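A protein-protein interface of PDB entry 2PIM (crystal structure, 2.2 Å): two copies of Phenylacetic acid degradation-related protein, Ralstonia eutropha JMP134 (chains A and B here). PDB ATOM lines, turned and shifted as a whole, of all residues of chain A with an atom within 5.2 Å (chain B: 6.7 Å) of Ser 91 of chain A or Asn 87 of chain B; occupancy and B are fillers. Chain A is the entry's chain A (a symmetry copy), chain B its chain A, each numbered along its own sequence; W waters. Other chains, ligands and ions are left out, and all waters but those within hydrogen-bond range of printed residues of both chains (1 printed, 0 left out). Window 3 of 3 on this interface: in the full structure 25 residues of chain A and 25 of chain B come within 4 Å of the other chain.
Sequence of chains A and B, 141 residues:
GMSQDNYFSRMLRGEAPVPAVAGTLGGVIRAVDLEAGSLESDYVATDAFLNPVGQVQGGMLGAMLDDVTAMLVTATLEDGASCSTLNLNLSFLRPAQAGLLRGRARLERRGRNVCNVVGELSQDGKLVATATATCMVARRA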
ATOM      1  N   ASN A  89       6.554 -32.087  16.977  1.00  0.00           N
ATOM      2  CA  ASN A  89       7.742 -31.284  16.951  1.00  0.00           C
ATOM      3  C   ASN A  89       7.367 -29.964  16.337  1.00  0.00           C
ATOM      4  O   ASN A  89       6.839 -29.933  15.227  1.00  0.00           O
ATOM      5  CB  ASN A  89       8.876 -31.954  16.147  1.00  0.00           C
ATOM      6  CG  ASN A  89      10.173 -31.126  16.174  1.00  0.00           C
ATOM      7  OD1 ASN A  89      10.416 -30.337  15.280  1.00  0.00           O
ATOM      8  ND2 ASN A  89      10.980 -31.296  17.212  1.00  0.00           N
ATOM      9  N   LEU A  90       7.661 -28.884  17.050  1.00  0.00           N
ATOM     10  CA  LEU A  90       7.243 -27.541  16.680  1.00  0.00           C
ATOM     11  C   LEU A  90       8.462 -26.698  16.387  1.00  0.00           C
ATOM     12  O   LEU A  90       9.403 -26.741  17.133  1.00  0.00           O
ATOM     13  CB  LEU A  90       6.527 -26.871  17.858  1.00  0.00           C
ATOM     14  CG  LEU A  90       5.299 -27.610  18.355  1.00  0.00           C
ATOM     15  CD1 LEU A  90       4.807 -26.930  19.645  1.00  0.00           C
ATOM     16  CD2 LEU A  90       4.198 -27.702  17.304  1.00  0.00           C
ATOM     17  N   SER A  91       8.418 -25.958  15.282  1.00  0.00           N
ATOM     18  CA  SER A  91       9.460 -25.053  14.889  1.00  0.00           C
ATOM     19  C   SER A  91       8.781 -23.713  14.793  1.00  0.00           C
ATOM     20  O   SER A  91       7.712 -23.580  14.152  1.00  0.00           O
ATOM     21  CB  SER A  91      10.083 -25.436  13.522  1.00  0.00           C
ATOM     22  OG  SER A  91      10.652 -26.732  13.538  1.00  0.00           O
ATOM     23  N   PHE A  92       9.431 -22.731  15.404  1.00  0.00           N
ATOM     24  CA  PHE A  92       8.943 -21.378  15.514  1.00  0.00           C
ATOM     25  C   PHE A  92       9.835 -20.510  14.658  1.00  0.00           C
ATOM     26  O   PHE A  92      11.012 -20.405  14.926  1.00  0.00           O
ATOM     27  CB  PHE A  92       9.004 -20.900  16.979  1.00  0.00           C
ATOM     28  CG  PHE A  92       8.258 -21.797  17.922  1.00  0.00           C
ATOM     29  CD1 PHE A  92       6.895 -21.968  17.779  1.00  0.00           C
ATOM     30  CD2 PHE A  92       8.917 -22.496  18.926  1.00  0.00           C
ATOM     31  CE1 PHE A  92       6.194 -22.821  18.600  1.00  0.00           C
ATOM     32  CE2 PHE A  92       8.203 -23.344  19.781  1.00  0.00           C
ATOM     33  CZ  PHE A  92       6.843 -23.513  19.601  1.00  0.00           C
ATOM     34  N   LEU A  93       9.234 -19.889  13.654  1.00  0.00           N
ATOM     35  CA  LEU A  93       9.922 -19.353  12.523  1.00  0.00           C
ATOM     36  C   LEU A  93       9.897 -17.845  12.588  1.00  0.00           C
ATOM     37  O   LEU A  93      10.928 -17.199  12.386  1.00  0.00           O
ATOM     38  CB  LEU A  93       9.196 -19.837  11.268  1.00  0.00           C
ATOM     39  CG  LEU A  93       9.718 -21.071  10.496  1.00  0.00           C
ATOM     40  CD1 LEU A  93      10.098 -22.218  11.340  1.00  0.00           C
ATOM     41  CD2 LEU A  93       8.698 -21.507   9.467  1.00  0.00           C
ATOM     42  N   VAL A 128       4.448 -18.616  10.382  1.00  0.00           N
ATOM     43  CA  VAL A 128       4.965 -18.310  11.713  1.00  0.00           C
ATOM     44  C   VAL A 128       5.555 -19.543  12.428  1.00  0.00           C
ATOM     45  O   VAL A 128       6.517 -19.419  13.215  1.00  0.00           O
ATOM     46  CB  VAL A 128       3.930 -17.558  12.555  1.00  0.00           C
ATOM     47  CG1 VAL A 128       3.612 -16.209  11.888  1.00  0.00           C
ATOM     48  CG2 VAL A 128       2.661 -18.335  12.746  1.00  0.00           C
ATOM     49  N   ALA A 129       4.988 -20.718  12.165  1.00  0.00           N
ATOM     50  CA  ALA A 129       5.423 -21.906  12.818  1.00  0.00           C
ATOM     51  C   ALA A 129       5.064 -23.116  11.976  1.00  0.00           C
ATOM     52  O   ALA A 129       4.095 -23.075  11.210  1.00  0.00           O
ATOM     53  CB  ALA A 129       4.776 -22.016  14.198  1.00  0.00           C
ATOM     54  N   THR A 130       5.864 -24.174  12.110  1.00  0.00           N
ATOM     55  CA  THR A 130       5.541 -25.465  11.512  1.00  0.00           C
ATOM     56  C   THR A 130       5.537 -26.579  12.542  1.00  0.00           C
ATOM     57  O   THR A 130       6.101 -26.435  13.629  1.00  0.00           O
ATOM     58  CB  THR A 130       6.525 -25.811  10.378  1.00  0.00           C
ATOM     59  OG1 THR A 130       7.830 -25.829  10.884  1.00  0.00           O
ATOM     60  CG2 THR A 130       6.483 -24.780   9.288  1.00  0.00           C
ATOM     61  N   ALA A 131       4.961 -27.707  12.148  1.00  0.00           N
ATOM     62  CA  ALA A 131       4.925 -28.893  12.950  1.00  0.00           C
ATOM     63  C   ALA A 131       5.039 -30.196  12.158  1.00  0.00           C
ATOM     64  O   ALA A 131       4.631 -30.293  10.998  1.00  0.00           O
ATOM     65  CB  ALA A 131       3.647 -28.956  13.730  1.00  0.00           C
ATOM     66  N   SER B  84      14.384 -16.837  23.319  1.00  0.00           N
ATOM     67  CA  SER B  84      13.622 -17.128  22.145  1.00  0.00           C
ATOM     68  C   SER B  84      13.644 -18.615  21.800  1.00  0.00           C
ATOM     69  O   SER B  84      14.654 -19.122  21.389  1.00  0.00           O
ATOM     70  CB  SER B  84      14.268 -16.320  21.036  1.00  0.00           C
ATOM     71  OG  SER B  84      13.562 -16.440  19.852  1.00  0.00           O
ATOM     72  N   THR B  85      12.529 -19.320  21.933  1.00  0.00           N
ATOM     73  CA  THR B  85      12.491 -20.754  21.639  1.00  0.00           C
ATOM     74  C   THR B  85      12.408 -21.065  20.134  1.00  0.00           C
ATOM     75  O   THR B  85      11.516 -20.590  19.451  1.00  0.00           O
ATOM     76  CB  THR B  85      11.307 -21.415  22.357  1.00  0.00           C
ATOM     77  OG1 THR B  85      11.424 -21.200  23.776  1.00  0.00           O
ATOM     78  CG2 THR B  85      11.278 -22.893  22.117  1.00  0.00           C
ATOM     79  N   LEU B  86      13.317 -21.902  19.636  1.00  0.00           N
ATOM     80  CA  LEU B  86      13.464 -22.170  18.217  1.00  0.00           C
ATOM     81  C   LEU B  86      12.738 -23.436  17.847  1.00  0.00           C
ATOM     82  O   LEU B  86      12.109 -23.511  16.797  1.00  0.00           O
ATOM     83  CB  LEU B  86      14.930 -22.332  17.855  1.00  0.00           C
ATOM     84  CG  LEU B  86      15.826 -21.149  18.164  1.00  0.00           C
ATOM     85  CD1 LEU B  86      17.246 -21.446  17.699  1.00  0.00           C
ATOM     86  CD2 LEU B  86      15.347 -19.846  17.512  1.00  0.00           C
ATOM     87  N   ASN B  87      12.845 -24.440  18.703  1.00  0.00           N
ATOM     88  CA  ASN B  87      12.213 -25.728  18.496  1.00  0.00           C
ATOM     89  C   ASN B  87      11.749 -26.199  19.853  1.00  0.00           C
ATOM     90  O   ASN B  87      12.415 -25.892  20.870  1.00  0.00           O
ATOM     91  CB  ASN B  87      13.230 -26.754  17.910  1.00  0.00           C
ATOM     92  CG  ASN B  87      12.569 -28.089  17.477  1.00  0.00           C
ATOM     93  OD1 ASN B  87      12.573 -29.071  18.234  1.00  0.00           O
ATOM     94  ND2 ASN B  87      12.066 -28.139  16.201  1.00  0.00           N
ATOM     95  N   LEU B  88      10.610 -26.909  19.863  1.00  0.00           N
ATOM     96  CA  LEU B  88      10.080 -27.560  21.054  1.00  0.00           C
ATOM     97  C   LEU B  88       9.527 -28.938  20.626  1.00  0.00           C
ATOM     98  O   LEU B  88       8.685 -29.009  19.774  1.00  0.00           O
ATOM     99  CB  LEU B  88       8.951 -26.714  21.633  1.00  0.00           C
ATOM    100  CG  LEU B  88       8.209 -27.133  22.908  1.00  0.00           C
ATOM    101  CD1 LEU B  88       9.129 -27.284  24.095  1.00  0.00           C
ATOM    102  CD2 LEU B  88       7.151 -26.109  23.211  1.00  0.00           C
ATOM    103  N   ASN B  89      10.069 -30.019  21.168  1.00  0.00           N
ATOM    104  CA  ASN B  89       9.624 -31.338  20.825  1.00  0.00           C
ATOM    105  C   ASN B  89       8.856 -31.864  22.006  1.00  0.00           C
ATOM    106  O   ASN B  89       9.386 -31.895  23.116  1.00  0.00           O
ATOM    107  CB  ASN B  89      10.801 -32.276  20.483  1.00  0.00           C
ATOM    108  CG  ASN B  89      10.323 -33.674  20.050  1.00  0.00           C
ATOM    109  OD1 ASN B  89      10.240 -34.574  20.866  1.00  0.00           O
ATOM    110  ND2 ASN B  89       9.991 -33.834  18.777  1.00  0.00           N
ATOM    111  N   THR B 132      11.564 -31.215  25.049  1.00  0.00           N
ATOM    112  CA  THR B 132      12.891 -30.710  24.829  1.00  0.00           C
ATOM    113  C   THR B 132      12.752 -29.385  24.098  1.00  0.00           C
ATOM    114  O   THR B 132      12.136 -29.325  23.031  1.00  0.00           O
ATOM    115  CB  THR B 132      13.669 -31.746  23.936  1.00  0.00           C
ATOM    116  OG1 THR B 132      13.931 -32.918  24.721  1.00  0.00           O
ATOM    117  CG2 THR B 132      14.971 -31.169  23.433  1.00  0.00           C
ATOM    118  N   ALA B 133      13.335 -28.344  24.648  1.00  0.00           N
ATOM    119  CA  ALA B 133      13.344 -27.020  24.048  1.00  0.00           C
ATOM    120  C   ALA B 133      14.743 -26.629  23.672  1.00  0.00           C
ATOM    121  O   ALA B 133      15.673 -26.818  24.452  1.00  0.00           O
ATOM    122  CB  ALA B 133      12.820 -26.000  25.033  1.00  0.00           C
ATOM    123  N   THR B 134      14.888 -26.099  22.462  1.00  0.00           N
ATOM    124  CA  THR B 134      16.104 -25.434  22.015  1.00  0.00           C
ATOM    125  C   THR B 134      15.834 -23.955  21.928  1.00  0.00           C
ATOM    126  O   THR B 134      14.969 -23.551  21.171  1.00  0.00           O
ATOM    127  CB  THR B 134      16.494 -25.948  20.628  1.00  0.00           C
ATOM    128  OG1 THR B 134      16.624 -27.358  20.706  1.00  0.00           O
ATOM    129  CG2 THR B 134      17.765 -25.329  20.158  1.00  0.00           C
ATOM    130  N   CYS B 135      16.563 -23.171  22.709  1.00  0.00           N
ATOM    131  CA  CYS B 135      16.304 -21.754  22.906  1.00  0.00           C
ATOM    132  C   CYS B 135      17.541 -20.968  22.574  1.00  0.00           C
ATOM    133  O   CYS B 135      18.631 -21.405  22.870  1.00  0.00           O
ATOM    134  CB  CYS B 135      15.968 -21.455  24.369  1.00  0.00           C
ATOM    135  SG  CYS B 135      14.585 -22.401  24.970  1.00  0.00           S
HETATM  136  O   HOH W   1      13.550 -21.692  14.459  1.00  0.00           O
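Asn 89 of chain B touches its own counterpart, Asn 89 of chain A.
ND2 of Asn 87 of chain B sits at hydrogen-bond distance from O of Leu 90 of chain A (3.1 Å). The side-chain amide nitrogen of Asn 89 of chain B lies close to the side-chain amide nitrogen of Asn 89 of chain A, at 3.1 Å. The backbone carbonyl oxygen (O) of Leu 88 of chain B sits at hydrogen-bond distance from the backbone NH (N) of Leu 90 of chain A, at 2.9 Å. The side-chain amide nitrogen (ND2) of Asn 87 of chain B sits at hydrogen-bond distance from the side-chain amide oxygen (OD1) of Asn 89 of chain A. The side-chain amide nitrogen of Asn 87 of chain B is in hydrogen-bond range of the side-chain hydroxyl of Ser 91 of chain A. The backbone NH of Phe 92 of chain A sits at hydrogen-bond distance from the backbone carbonyl oxygen of Leu 86 of chain B (3.1 Å).
Of the 9 printed residues of chain A, 4 touch a printed residue of chain B. Of the 10 printed residues of chain B, 5 touch a printed residue of chain A. Printed residues of chain B that touch a printed residue of chain A: Thr 85, Leu 86, Asn 87, Leu 88 and Asn 89. Hydrophobic or aromatic side chains of chain B that line the printed part of chain A: Leu 88. Among the printed residues, 10 pairs touch across the chains. Among the printed residues, no Asp or Glu carboxylate lies within 4 Å of a Lys or Arg side-chain nitrogen of the other chain.
N of Leu 86 of chain B sits at hydrogen-bond distance from O of Thr 134 of chain B (2.8 Å). The backbone carbonyl oxygen (O) of Asn 87 of chain B is in hydrogen-bond range of the backbone NH (N) of Thr 134 of chain B, 2.9 Å away. N of Asn 89 of chain B is in hydrogen-bond range of O of Thr 132 of chain B (2.9 Å). SG of Cys 135 of chain B sits at hydrogen-bond distance from OG1 of Thr 85 of chain B (3.6 Å). The backbone NH of Thr 130 of chain A sits at hydrogen-bond distance from the backbone carbonyl oxygen of Ser 91 of chain A.
Printed residues of chain B within 4 Å of Leu 90 of chain A: Asn 87 and Leu 88. Of the printed residues of chain B, Ser 91 of chain A touches Leu 86 and Asn 87. Of the printed residues of chain B, Phe 92 of chain A touches Thr 85, Leu 86 and Leu 88. Leu 93 of chain A touches none of the printed residues of chain B. Ala 129 of chain A touches none of the printed residues of chain B. Of the printed residues of chain A, Asn 87 of chain B touches Asn 89 (2.9 Å), Leu 90 (3.1 Å) and Ser 91 (3.3 Å). The nearest residue of chain A that does not touch Asn 87 of chain B is Phe 92 of chain A (4.4 Å). The nearest printed residue of chain B that does not touch Phe 92 of chain A is Asn 87 of chain B (4.4 Å).
Water W1 bridges O of Phe 92 of chain A and O of Leu 86 of chain B.
CA of Asn 89 of chain A touches O of Leu 88 of chain B (3.7 Å). CA of Ser 91 of chain A touches O of Leu 86 of chain B (3.6 Å). Thr 85 of chain B touches Phe 92 of chain A (O to CD2, 3.3 Å). Phe 92 of chain A touches Leu 88 of chain B (CE2 to CB, 3.9 Å).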
